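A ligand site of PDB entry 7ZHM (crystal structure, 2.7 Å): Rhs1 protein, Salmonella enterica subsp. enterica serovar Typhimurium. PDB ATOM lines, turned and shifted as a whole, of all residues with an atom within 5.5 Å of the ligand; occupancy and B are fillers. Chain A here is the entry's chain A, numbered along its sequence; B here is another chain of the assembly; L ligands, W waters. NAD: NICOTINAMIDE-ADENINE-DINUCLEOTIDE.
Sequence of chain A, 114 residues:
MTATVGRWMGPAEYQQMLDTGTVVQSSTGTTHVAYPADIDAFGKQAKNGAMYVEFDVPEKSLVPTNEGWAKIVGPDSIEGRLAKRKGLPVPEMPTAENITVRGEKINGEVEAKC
Residues that only touch the ligand: Phe 42 (3.3 Å), Asn 22 of chain B (3.3 Å), Ser 25 of chain B (3.4 Å), Asp 46 of chain B (3.4 Å), Met 9 (3.5 Å), Thr 28 (3.6 Å), Val 33 (3.6 Å), Val 24 of chain A (3.8 Å), Ala 34 (3.8 Å), Leu 24 of chain B (3.8 Å) and Trp 69 (3.8 Å).
Hydrophobic or aromatic side chains within 4 Å of the ligand: Trp 8, Met 9, Val 24 of chain A, His 32, Phe 42, Trp 69, Leu 24 of chain B and Trp 44 of chain B.
22 residues have an atom within 4 Å of the ligand: Arg 7, Trp 8, Met 9, Gly 10, Glu 13, Val 24 of chain A, Gln 25 of chain A, Ser 26, Ser 27 of chain A, Thr 28, His 32, Val 33, Ala 34, Phe 42, Trp 69, Asn 22 of chain B, Leu 24 of chain B, Ser 25 of chain B, Trp 44 of chain B, Asp 46 of chain B, Ser 48 of chain B and Arg 66 of chain B.
The nearest printed residue that does not touch the ligand is Gln 45 (4.5 Å).
Water W2 bridges N3A of the ligand and N of Glu 13.
Water W1 lies within hydrogen-bond range of N of His 32 (2.7 Å), O1A of the ligand (2.8 Å), NH1 of Arg 7 (3.1 Å) and O of Thr 30 (3.3 Å).
Water W3 bridges an oxygen (O7N) of the ligand (2.8 Å) and the backbone carbonyl oxygen of Gly 6 (3.1 Å).
OE2 of Glu 13 lies within salt-bridge range of NE of Arg 7 (2.8 Å).
NH1 of Arg 7 sits at hydrogen-bond distance from O of His 32 (2.8 Å).
OD1 of Asp 46 of chain B lies within hydrogen-bond range of OG of Ser 48 of chain B (2.8 Å).
The side-chain hydroxyl (OG) of Ser 26 is in hydrogen-bond range of the side-chain hydroxyl (OG1) of Thr 28 (2.8 Å).
N of Ser 26 sits at hydrogen-bond distance from OG1 of Thr 31, 2.8 Å away.
The side-chain amide nitrogen of Asn 22 of chain B lies within hydrogen-bond range of the side-chain hydroxyl of Ser 27 of chain A (3.0 Å).
OG1 of Thr 28 is in hydrogen-bond range of O of Thr 30 (3.0 Å).
The backbone carbonyl oxygen (O) of Gly 6 lies within hydrogen-bond range of the backbone NH (N) of Ala 34, 2.8 Å away.
OE1 of Glu 13 lies within hydrogen-bond range of O2B of the ligand (2.5 Å).
An oxygen (O2D) of the ligand sits at hydrogen-bond distance from a ring nitrogen (ND1) of His 32.
The guanidinium group (NH1) of Arg 7 is in salt-bridge range of an oxygen (O1N) of the ligand, 2.7 Å away.
OG of Ser 48 of chain B is in hydrogen-bond range of O3D of the ligand, at 2.7 Å.
The backbone NH (N) of Trp 8 lies within hydrogen-bond range of an oxygen (O7N) of the ligand (2.7 Å).
O of Trp 8 sits at hydrogen-bond distance from N7N of the ligand, 3.0 Å away.
OG of Ser 26 sits at hydrogen-bond distance from O1A of the ligand (2.7 Å).
NE of Arg 66 of chain B is in hydrogen-bond range of O2D of the ligand.
The backbone NH of Gly 10 lies within hydrogen-bond range of an oxygen (O2B) of the ligand (3.0 Å).
The indole nitrogen of Trp 44 of chain B is in hydrogen-bond range of an oxygen (O3) of the ligand, 3.1 Å away.
N7A of the ligand sits at hydrogen-bond distance from N of Ser 27 of chain A.
A nitrogen (N7A) of the ligand sits at hydrogen-bond distance from the side-chain hydroxyl of Ser 27 of chain A.
A nitrogen (N6A) of the ligand lies within hydrogen-bond range of the backbone carbonyl oxygen (O) of Gln 25 of chain A (3.2 Å).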
ATOM      1  N   GLY A   6     -21.792  19.841 -10.650  1.00  0.00           N
ATOM      2  CA  GLY A   6     -22.023  19.928 -12.082  1.00  0.00           C
ATOM      3  C   GLY A   6     -20.982  19.119 -12.820  1.00  0.00           C
ATOM      4  O   GLY A   6     -19.839  19.024 -12.368  1.00  0.00           O
ATOM      5  N   ARG A   7     -21.386  18.529 -13.955  1.00  0.00           N
ATOM      6  CA  ARG A   7     -20.510  17.663 -14.784  1.00  0.00           C
ATOM      7  C   ARG A   7     -20.888  17.791 -16.260  1.00  0.00           C
ATOM      8  O   ARG A   7     -22.060  17.591 -16.584  1.00  0.00           O
ATOM      9  CB  ARG A   7     -20.589  16.203 -14.327  1.00  0.00           C
ATOM     10  CG  ARG A   7     -19.555  15.305 -14.980  1.00  0.00           C
ATOM     11  CD  ARG A   7     -19.451  13.921 -14.373  1.00  0.00           C
ATOM     12  NE  ARG A   7     -18.945  12.968 -15.339  1.00  0.00           N
ATOM     13  CZ  ARG A   7     -17.678  12.868 -15.750  1.00  0.00           C
ATOM     14  NH1 ARG A   7     -16.743  13.674 -15.269  1.00  0.00           N
ATOM     15  NH2 ARG A   7     -17.342  11.952 -16.648  1.00  0.00           N
ATOM     16  N   TRP A   8     -19.903  18.108 -17.104  1.00  0.00           N
ATOM     17  CA  TRP A   8     -20.008  18.014 -18.546  1.00  0.00           C
ATOM     18  C   TRP A   8     -19.800  16.555 -18.931  1.00  0.00           C
ATOM     19  O   TRP A   8     -18.759  15.989 -18.648  1.00  0.00           O
ATOM     20  CB  TRP A   8     -18.939  18.884 -19.217  1.00  0.00           C
ATOM     21  CG  TRP A   8     -19.191  20.368 -19.136  1.00  0.00           C
ATOM     22  CD1 TRP A   8     -18.677  21.240 -18.226  1.00  0.00           C
ATOM     23  CD2 TRP A   8     -20.018  21.144 -20.004  1.00  0.00           C
ATOM     24  NE1 TRP A   8     -19.130  22.510 -18.468  1.00  0.00           N
ATOM     25  CE2 TRP A   8     -19.956  22.484 -19.570  1.00  0.00           C
ATOM     26  CE3 TRP A   8     -20.817  20.843 -21.120  1.00  0.00           C
ATOM     27  CZ2 TRP A   8     -20.652  23.512 -20.191  1.00  0.00           C
ATOM     28  CZ3 TRP A   8     -21.500  21.871 -21.747  1.00  0.00           C
ATOM     29  CH2 TRP A   8     -21.417  23.185 -21.280  1.00  0.00           C
ATOM     30  N   MET A   9     -20.838  15.960 -19.548  1.00  0.00           N
ATOM     31  CA  MET A   9     -20.841  14.549 -19.926  1.00  0.00           C
ATOM     32  C   MET A   9     -21.486  14.346 -21.288  1.00  0.00           C
ATOM     33  O   MET A   9     -22.232  15.211 -21.777  1.00  0.00           O
ATOM     34  CB  MET A   9     -21.581  13.732 -18.870  1.00  0.00           C
ATOM     35  CG  MET A   9     -23.061  14.080 -18.732  1.00  0.00           C
ATOM     36  SD  MET A   9     -23.902  13.214 -17.383  1.00  0.00           S
ATOM     37  CE  MET A   9     -23.044  13.894 -15.970  1.00  0.00           C
ATOM     38  N   GLY A  10     -21.217  13.190 -21.887  1.00  0.00           N
ATOM     39  CA  GLY A  10     -21.809  12.799 -23.158  1.00  0.00           C
ATOM     40  C   GLY A  10     -23.225  12.240 -23.008  1.00  0.00           C
ATOM     41  O   GLY A  10     -23.637  11.859 -21.913  1.00  0.00           O
ATOM     42  N   ALA A  12     -24.593   9.355 -23.685  1.00  0.00           N
ATOM     43  CA  ALA A  12     -24.631   7.987 -23.159  1.00  0.00           C
ATOM     44  C   ALA A  12     -24.505   7.942 -21.634  1.00  0.00           C
ATOM     45  O   ALA A  12     -25.203   7.179 -20.970  1.00  0.00           O
ATOM     46  CB  ALA A  12     -23.565   7.130 -23.816  1.00  0.00           C
ATOM     47  N   GLU A  13     -23.613   8.769 -21.076  1.00  0.00           N
ATOM     48  CA  GLU A  13     -23.431   8.854 -19.634  1.00  0.00           C
ATOM     49  C   GLU A  13     -24.683   9.416 -18.967  1.00  0.00           C
ATOM     50  O   GLU A  13     -25.157   8.866 -17.982  1.00  0.00           O
ATOM     51  CB  GLU A  13     -22.213   9.711 -19.253  1.00  0.00           C
ATOM     52  CG  GLU A  13     -21.888   9.664 -17.767  1.00  0.00           C
ATOM     53  CD  GLU A  13     -20.700  10.513 -17.364  1.00  0.00           C
ATOM     54  OE1 GLU A  13     -19.716  10.589 -18.130  1.00  0.00           O
ATOM     55  OE2 GLU A  13     -20.738  11.091 -16.254  1.00  0.00           O
ATOM     56  N   GLN A  16     -27.491   6.913 -18.876  1.00  0.00           N
ATOM     57  CA  GLN A  16     -27.215   5.894 -17.871  1.00  0.00           C
ATOM     58  C   GLN A  16     -27.475   6.432 -16.463  1.00  0.00           C
ATOM     59  O   GLN A  16     -28.083   5.756 -15.634  1.00  0.00           O
ATOM     60  CB  GLN A  16     -25.788   5.374 -18.005  1.00  0.00           C
ATOM     61  CG  GLN A  16     -25.522   4.126 -17.178  1.00  0.00           C
ATOM     62  CD  GLN A  16     -24.068   3.675 -17.256  1.00  0.00           C
ATOM     63  OE1 GLN A  16     -23.496   3.585 -18.340  1.00  0.00           O
ATOM     64  NE2 GLN A  16     -23.487   3.362 -16.097  1.00  0.00           N
ATOM     65  N   VAL A  24     -22.414   7.755 -12.848  1.00  0.00           N
ATOM     66  CA  VAL A  24     -21.652   6.811 -13.647  1.00  0.00           C
ATOM     67  C   VAL A  24     -20.166   6.986 -13.323  1.00  0.00           C
ATOM     68  O   VAL A  24     -19.678   8.104 -13.274  1.00  0.00           O
ATOM     69  CB  VAL A  24     -21.881   7.007 -15.159  1.00  0.00           C
ATOM     70  CG1 VAL A  24     -21.007   6.064 -15.968  1.00  0.00           C
ATOM     71  CG2 VAL A  24     -23.336   6.810 -15.501  1.00  0.00           C
ATOM     72  N   GLN A  25     -19.472   5.870 -13.092  1.00  0.00           N
ATOM     73  CA  GLN A  25     -18.039   5.867 -12.873  1.00  0.00           C
ATOM     74  C   GLN A  25     -17.328   6.067 -14.202  1.00  0.00           C
ATOM     75  O   GLN A  25     -17.526   5.307 -15.143  1.00  0.00           O
ATOM     76  CB  GLN A  25     -17.587   4.554 -12.234  1.00  0.00           C
ATOM     77  CG  GLN A  25     -16.130   4.577 -11.780  1.00  0.00           C
ATOM     78  CD  GLN A  25     -15.735   3.370 -10.961  1.00  0.00           C
ATOM     79  OE1 GLN A  25     -15.366   3.491  -9.786  1.00  0.00           O
ATOM     80  NE2 GLN A  25     -15.817   2.197 -11.568  1.00  0.00           N
ATOM     81  N   SER A  26     -16.496   7.112 -14.275  1.00  0.00           N
ATOM     82  CA  SER A  26     -15.634   7.362 -15.421  1.00  0.00           C
ATOM     83  C   SER A  26     -14.830   6.105 -15.745  1.00  0.00           C
ATOM     84  O   SER A  26     -14.463   5.353 -14.861  1.00  0.00           O
ATOM     85  CB  SER A  26     -14.686   8.524 -15.126  1.00  0.00           C
ATOM     86  OG  SER A  26     -13.768   8.717 -16.186  1.00  0.00           O
ATOM     87  N   SER A  27     -14.554   5.897 -17.040  1.00  0.00           N
ATOM     88  CA  SER A  27     -13.693   4.805 -17.485  1.00  0.00           C
ATOM     89  C   SER A  27     -12.216   5.040 -17.097  1.00  0.00           C
ATOM     90  O   SER A  27     -11.381   4.166 -17.300  1.00  0.00           O
ATOM     91  CB  SER A  27     -13.839   4.569 -18.989  1.00  0.00           C
ATOM     92  OG  SER A  27     -13.747   5.775 -19.731  1.00  0.00           O
ATOM     93  N   THR A  28     -11.923   6.231 -16.537  1.00  0.00           N
ATOM     94  CA  THR A  28     -10.627   6.508 -15.913  1.00  0.00           C
ATOM     95  C   THR A  28     -10.512   5.930 -14.502  1.00  0.00           C
ATOM     96  O   THR A  28      -9.404   5.805 -13.983  1.00  0.00           O
ATOM     97  CB  THR A  28     -10.345   8.032 -15.829  1.00  0.00           C
ATOM     98  OG1 THR A  28     -11.268   8.663 -14.942  1.00  0.00           O
ATOM     99  CG2 THR A  28     -10.403   8.666 -17.204  1.00  0.00           C
ATOM    100  N   THR A  30     -12.094   7.352 -11.817  1.00  0.00           N
ATOM    101  CA  THR A  30     -12.537   8.433 -10.952  1.00  0.00           C
ATOM    102  C   THR A  30     -13.339   9.451 -11.767  1.00  0.00           C
ATOM    103  O   THR A  30     -12.847  10.012 -12.746  1.00  0.00           O
ATOM    104  CB  THR A  30     -11.351   9.142 -10.269  1.00  0.00           C
ATOM    105  OG1 THR A  30     -10.424   8.159  -9.779  1.00  0.00           O
ATOM    106  CG2 THR A  30     -11.827  10.012  -9.116  1.00  0.00           C
ATOM    107  N   THR A  31     -14.582   9.695 -11.335  1.00  0.00           N
ATOM    108  CA  THR A  31     -15.443  10.682 -11.941  1.00  0.00           C
ATOM    109  C   THR A  31     -15.155  12.028 -11.286  1.00  0.00           C
ATOM    110  O   THR A  31     -15.232  12.156 -10.074  1.00  0.00           O
ATOM    111  CB  THR A  31     -16.921  10.306 -11.777  1.00  0.00           C
ATOM    112  OG1 THR A  31     -17.147   9.029 -12.384  1.00  0.00           O
ATOM    113  CG2 THR A  31     -17.827  11.344 -12.441  1.00  0.00           C
ATOM    114  N   HIS A  32     -14.809  13.023 -12.114  1.00  0.00           N
ATOM    115  CA  HIS A  32     -14.547  14.372 -11.644  1.00  0.00           C
ATOM    116  C   HIS A  32     -15.788  15.224 -11.884  1.00  0.00           C
ATOM    117  O   HIS A  32     -16.499  15.026 -12.860  1.00  0.00           O
ATOM    118  CB  HIS A  32     -13.333  14.952 -12.378  1.00  0.00           C
ATOM    119  CG  HIS A  32     -12.033  14.350 -11.954  1.00  0.00           C
ATOM    120  ND1 HIS A  32     -10.816  14.937 -12.231  1.00  0.00           N
ATOM    121  CD2 HIS A  32     -11.757  13.214 -11.258  1.00  0.00           C
ATOM    122  CE1 HIS A  32      -9.845  14.189 -11.734  1.00  0.00           C
ATOM    123  NE2 HIS A  32     -10.395  13.134 -11.144  1.00  0.00           N
ATOM    124  N   VAL A  33     -16.053  16.137 -10.945  1.00  0.00           N
ATOM    125  CA  VAL A  33     -17.182  17.057 -11.019  1.00  0.00           C
ATOM    126  C   VAL A  33     -16.725  18.434 -10.583  1.00  0.00           C
ATOM    127  O   VAL A  33     -15.714  18.555  -9.889  1.00  0.00           O
ATOM    128  CB  VAL A  33     -18.345  16.605 -10.108  1.00  0.00           C
ATOM    129  CG1 VAL A  33     -18.811  15.206 -10.490  1.00  0.00           C
ATOM    130  CG2 VAL A  33     -17.946  16.658  -8.639  1.00  0.00           C
ATOM    131  N   ALA A  34     -17.457  19.461 -11.002  1.00  0.00           N
ATOM    132  CA  ALA A  34     -17.262  20.819 -10.528  1.00  0.00           C
ATOM    133  C   ALA A  34     -17.917  20.950  -9.157  1.00  0.00           C
ATOM    134  O   ALA A  34     -19.057  20.523  -8.969  1.00  0.00           O
ATOM    135  CB  ALA A  34     -17.849  21.826 -11.504  1.00  0.00           C
ATOM    136  N   PHE A  42     -15.361  24.124 -16.285  1.00  0.00           N
ATOM    137  CA  PHE A  42     -14.736  23.145 -17.167  1.00  0.00           C
ATOM    138  C   PHE A  42     -15.408  23.022 -18.530  1.00  0.00           C
ATOM    139  O   PHE A  42     -15.261  22.020 -19.232  1.00  0.00           O
ATOM    140  CB  PHE A  42     -14.645  21.796 -16.450  1.00  0.00           C
ATOM    141  CG  PHE A  42     -13.786  21.843 -15.219  1.00  0.00           C
ATOM    142  CD1 PHE A  42     -12.399  21.730 -15.329  1.00  0.00           C
ATOM    143  CD2 PHE A  42     -14.345  22.078 -13.977  1.00  0.00           C
ATOM    144  CE1 PHE A  42     -11.594  21.798 -14.209  1.00  0.00           C
ATOM    145  CE2 PHE A  42     -13.535  22.158 -12.846  1.00  0.00           C
ATOM    146  CZ  PHE A  42     -12.162  22.013 -12.968  1.00  0.00           C
ATOM    147  N   GLN A  45     -13.029  23.191 -22.238  1.00  0.00           N
ATOM    148  CA  GLN A  45     -12.436  21.970 -22.772  1.00  0.00           C
ATOM    149  C   GLN A  45     -13.426  20.855 -23.079  1.00  0.00           C
ATOM    150  O   GLN A  45     -13.048  19.827 -23.652  1.00  0.00           O
ATOM    151  CB  GLN A  45     -11.343  21.431 -21.831  1.00  0.00           C
ATOM    152  CG  GLN A  45     -11.803  21.138 -20.410  1.00  0.00           C
ATOM    153  CD  GLN A  45     -11.186  22.089 -19.393  1.00  0.00           C
ATOM    154  OE1 GLN A  45     -11.686  23.202 -19.186  1.00  0.00           O
ATOM    155  NE2 GLN A  45     -10.111  21.646 -18.755  1.00  0.00           N
ATOM    156  N   TRP A  69     -12.949  21.835  -8.486  1.00  0.00           N
ATOM    157  CA  TRP A  69     -13.389  20.481  -8.832  1.00  0.00           C
ATOM    158  C   TRP A  69     -13.243  19.527  -7.648  1.00  0.00           C
ATOM    159  O   TRP A  69     -12.590  19.857  -6.660  1.00  0.00           O
ATOM    160  CB  TRP A  69     -12.624  19.941 -10.045  1.00  0.00           C
ATOM    161  CG  TRP A  69     -11.155  19.786  -9.834  1.00  0.00           C
ATOM    162  CD1 TRP A  69     -10.196  20.767  -9.944  1.00  0.00           C
ATOM    163  CD2 TRP A  69     -10.460  18.586  -9.482  1.00  0.00           C
ATOM    164  NE1 TRP A  69      -8.958  20.252  -9.677  1.00  0.00           N
ATOM    165  CE2 TRP A  69      -9.089  18.918  -9.389  1.00  0.00           C
ATOM    166  CE3 TRP A  69     -10.858  17.272  -9.228  1.00  0.00           C
ATOM    167  CZ2 TRP A  69      -8.113  17.973  -9.058  1.00  0.00           C
ATOM    168  CZ3 TRP A  69      -9.891  16.327  -8.901  1.00  0.00           C
ATOM    169  CH2 TRP A  69      -8.543  16.687  -8.811  1.00  0.00           C
ATOM    170  N   ASN B  22     -14.366   6.768 -25.645  1.00  0.00           N
ATOM    171  CA  ASN B  22     -15.749   7.194 -25.469  1.00  0.00           C
ATOM    172  C   ASN B  22     -16.143   8.109 -26.616  1.00  0.00           C
ATOM    173  O   ASN B  22     -15.270   8.693 -27.282  1.00  0.00           O
ATOM    174  CB  ASN B  22     -15.942   7.896 -24.124  1.00  0.00           C
ATOM    175  CG  ASN B  22     -15.759   6.964 -22.929  1.00  0.00           C
ATOM    176  OD1 ASN B  22     -16.640   6.166 -22.616  1.00  0.00           O
ATOM    177  ND2 ASN B  22     -14.621   7.084 -22.258  1.00  0.00           N
ATOM    178  N   LEU B  24     -17.001  11.056 -27.030  1.00  0.00           N
ATOM    179  CA  LEU B  24     -16.443  12.409 -27.040  1.00  0.00           C
ATOM    180  C   LEU B  24     -14.969  12.504 -26.644  1.00  0.00           C
ATOM    181  O   LEU B  24     -14.283  13.435 -27.064  1.00  0.00           O
ATOM    182  CB  LEU B  24     -17.283  13.325 -26.148  1.00  0.00           C
ATOM    183  CG  LEU B  24     -18.786  13.415 -26.452  1.00  0.00           C
ATOM    184  CD1 LEU B  24     -19.445  14.438 -25.546  1.00  0.00           C
ATOM    185  CD2 LEU B  24     -19.057  13.760 -27.914  1.00  0.00           C
ATOM    186  N   SER B  25     -14.475  11.548 -25.853  1.00  0.00           N
ATOM    187  CA  SER B  25     -13.114  11.580 -25.320  1.00  0.00           C
ATOM    188  C   SER B  25     -12.324  10.297 -25.548  1.00  0.00           C
ATOM    189  O   SER B  25     -12.828   9.192 -25.367  1.00  0.00           O
ATOM    190  CB  SER B  25     -13.126  11.895 -23.814  1.00  0.00           C
ATOM    191  OG  SER B  25     -11.819  11.924 -23.226  1.00  0.00           O
ATOM    192  N   SER B  27      -8.762   8.793 -23.769  1.00  0.00           N
ATOM    193  CA  SER B  27      -7.849   8.966 -22.643  1.00  0.00           C
ATOM    194  C   SER B  27      -6.979   7.726 -22.454  1.00  0.00           C
ATOM    195  O   SER B  27      -7.233   6.666 -23.027  1.00  0.00           O
ATOM    196  CB  SER B  27      -8.607   9.326 -21.357  1.00  0.00           C
ATOM    197  OG  SER B  27      -9.626   8.383 -21.048  1.00  0.00           O
ATOM    198  N   TRP B  44      -5.675  12.948 -20.665  1.00  0.00           N
ATOM    199  CA  TRP B  44      -6.816  13.140 -21.554  1.00  0.00           C
ATOM    200  C   TRP B  44      -6.414  13.825 -22.848  1.00  0.00           C
ATOM    201  O   TRP B  44      -5.374  14.477 -22.934  1.00  0.00           O
ATOM    202  CB  TRP B  44      -7.865  14.013 -20.861  1.00  0.00           C
ATOM    203  CG  TRP B  44      -8.634  13.353 -19.762  1.00  0.00           C
ATOM    204  CD1 TRP B  44      -9.794  12.638 -19.879  1.00  0.00           C
ATOM    205  CD2 TRP B  44      -8.313  13.374 -18.363  1.00  0.00           C
ATOM    206  NE1 TRP B  44     -10.212  12.206 -18.649  1.00  0.00           N
ATOM    207  CE2 TRP B  44      -9.316  12.646 -17.697  1.00  0.00           C
ATOM    208  CE3 TRP B  44      -7.272  13.939 -17.610  1.00  0.00           C
ATOM    209  CZ2 TRP B  44      -9.314  12.456 -16.321  1.00  0.00           C
ATOM    210  CZ3 TRP B  44      -7.276  13.757 -16.248  1.00  0.00           C
ATOM    211  CH2 TRP B  44      -8.290  13.015 -15.607  1.00  0.00           C
ATOM    212  N   ASP B  46      -7.855  16.368 -24.005  1.00  0.00           N
ATOM    213  CA  ASP B  46      -8.111  17.796 -23.821  1.00  0.00           C
ATOM    214  C   ASP B  46      -6.917  18.576 -23.200  1.00  0.00           C
ATOM    215  O   ASP B  46      -7.094  19.680 -22.687  1.00  0.00           O
ATOM    216  CB  ASP B  46      -9.401  18.017 -22.991  1.00  0.00           C
ATOM    217  CG  ASP B  46      -9.217  17.758 -21.489  1.00  0.00           C
ATOM    218  OD1 ASP B  46      -8.215  17.117 -21.092  1.00  0.00           O
ATOM    219  OD2 ASP B  46     -10.086  18.193 -20.704  1.00  0.00           O
ATOM    220  N   SER B  48      -4.941  17.799 -20.564  1.00  0.00           N
ATOM    221  CA  SER B  48      -4.875  17.773 -19.110  1.00  0.00           C
ATOM    222  C   SER B  48      -4.448  16.380 -18.665  1.00  0.00           C
ATOM    223  O   SER B  48      -4.529  15.433 -19.455  1.00  0.00           O
ATOM    224  CB  SER B  48      -6.228  18.146 -18.479  1.00  0.00           C
ATOM    225  OG  SER B  48      -7.157  17.079 -18.540  1.00  0.00           O
ATOM    226  N   CYS B  49      -3.965  16.278 -17.434  1.00  0.00           N
ATOM    227  CA  CYS B  49      -3.563  15.008 -16.842  1.00  0.00           C
ATOM    228  C   CYS B  49      -3.688  15.040 -15.320  1.00  0.00           C
ATOM    229  O   CYS B  49      -3.727  16.119 -14.716  1.00  0.00           O
ATOM    230  CB  CYS B  49      -2.142  14.628 -17.259  1.00  0.00           C
ATOM    231  SG  CYS B  49      -0.854  15.759 -16.671  1.00  0.00           S
ATOM    232  N   ARG B  66      -3.480  17.695 -10.326  1.00  0.00           N
ATOM    233  CA  ARG B  66      -4.138  17.881 -11.651  1.00  0.00           C
ATOM    234  C   ARG B  66      -3.371  18.951 -12.439  1.00  0.00           C
ATOM    235  O   ARG B  66      -3.214  20.054 -11.900  1.00  0.00           O
ATOM    236  CB  ARG B  66      -5.601  18.290 -11.515  1.00  0.00           C
ATOM    237  CG  ARG B  66      -6.304  18.453 -12.855  1.00  0.00           C
ATOM    238  CD  ARG B  66      -7.775  18.794 -12.767  1.00  0.00           C
ATOM    239  NE  ARG B  66      -8.305  18.916 -14.129  1.00  0.00           N
ATOM    240  CZ  ARG B  66      -8.179  19.986 -14.904  1.00  0.00           C
ATOM    241  NH1 ARG B  66      -7.556  21.071 -14.480  1.00  0.00           N
ATOM    242  NH2 ARG B  66      -8.688  19.968 -16.129  1.00  0.00           N
HETATM  243  PA  NAD L   1     -13.869  11.527 -18.363  1.00  0.00           P
HETATM  244  O1A NAD L   1     -14.458  11.220 -17.024  1.00  0.00           O
HETATM  245  O2A NAD L   1     -12.900  10.558 -18.945  1.00  0.00           O
HETATM  246  O5B NAD L   1     -15.064  11.796 -19.405  1.00  0.00           O
HETATM  247  C5B NAD L   1     -14.745  12.091 -20.797  1.00  0.00           C
HETATM  248  C4B NAD L   1     -15.923  11.737 -21.678  1.00  0.00           C
HETATM  249  O4B NAD L   1     -16.149  10.306 -21.622  1.00  0.00           O
HETATM  250  C3B NAD L   1     -17.262  12.386 -21.299  1.00  0.00           C
HETATM  251  O3B NAD L   1     -18.011  12.695 -22.471  1.00  0.00           O
HETATM  252  C2B NAD L   1     -17.930  11.296 -20.457  1.00  0.00           C
HETATM  253  O2B NAD L   1     -19.340  11.413 -20.455  1.00  0.00           O
HETATM  254  C1B NAD L   1     -17.465  10.045 -21.181  1.00  0.00           C
HETATM  255  N9A NAD L   1     -17.427   8.856 -20.334  1.00  0.00           N
HETATM  256  C8A NAD L   1     -16.442   8.522 -19.433  1.00  0.00           C
HETATM  257  N7A NAD L   1     -16.662   7.386 -18.818  1.00  0.00           N
HETATM  258  C5A NAD L   1     -17.853   6.933 -19.343  1.00  0.00           C
HETATM  259  C6A NAD L   1     -18.616   5.773 -19.095  1.00  0.00           C
HETATM  260  N6A NAD L   1     -18.263   4.837 -18.223  1.00  0.00           N
HETATM  261  N1A NAD L   1     -19.762   5.619 -19.796  1.00  0.00           N
HETATM  262  C2A NAD L   1     -20.115   6.575 -20.672  1.00  0.00           C
HETATM  263  N3A NAD L   1     -19.475   7.702 -20.986  1.00  0.00           N
HETATM  264  C4A NAD L   1     -18.338   7.827 -20.284  1.00  0.00           C
HETATM  265  O3  NAD L   1     -13.188  12.975 -18.293  1.00  0.00           O
HETATM  266  PN  NAD L   1     -13.755  14.443 -18.011  1.00  0.00           P
HETATM  267  O1N NAD L   1     -14.788  14.363 -16.927  1.00  0.00           O
HETATM  268  O2N NAD L   1     -14.143  15.062 -19.310  1.00  0.00           O
HETATM  269  O5D NAD L   1     -12.456  15.169 -17.427  1.00  0.00           O
HETATM  270  C5D NAD L   1     -11.468  15.740 -18.327  1.00  0.00           C
HETATM  271  C4D NAD L   1     -10.702  16.821 -17.606  1.00  0.00           C
HETATM  272  O4D NAD L   1     -11.624  17.801 -17.093  1.00  0.00           O
HETATM  273  C3D NAD L   1      -9.873  16.349 -16.389  1.00  0.00           C
HETATM  274  O3D NAD L   1      -8.671  17.111 -16.306  1.00  0.00           O
HETATM  275  C2D NAD L   1     -10.825  16.626 -15.224  1.00  0.00           C
HETATM  276  O2D NAD L   1     -10.159  16.811 -13.992  1.00  0.00           O
HETATM  277  C1D NAD L   1     -11.521  17.902 -15.674  1.00  0.00           C
HETATM  278  N1N NAD L   1     -12.881  18.056 -15.091  1.00  0.00           N
HETATM  279  C2N NAD L   1     -13.979  17.527 -15.731  1.00  0.00           C
HETATM  280  C3N NAD L   1     -15.254  17.808 -15.252  1.00  0.00           C
HETATM  281  C7N NAD L   1     -16.447  17.544 -16.142  1.00  0.00           C
HETATM  282  O7N NAD L   1     -17.396  18.318 -16.123  1.00  0.00           O
HETATM  283  N7N NAD L   1     -16.405  16.469 -16.919  1.00  0.00           N
HETATM  284  C4N NAD L   1     -15.386  18.338 -13.977  1.00  0.00           C
HETATM  285  C5N NAD L   1     -14.284  18.876 -13.348  1.00  0.00           C
HETATM  286  C6N NAD L   1     -13.039  18.713 -13.911  1.00  0.00           C
HETATM  287  O   HOH W   1     -13.922  12.455 -14.623  1.00  0.00           O
HETATM  288  O   HOH W   2     -20.810   9.101 -22.711  1.00  0.00           O
HETATM  289  O   HOH W   3     -18.321  20.517 -14.685  1.00  0.00           O
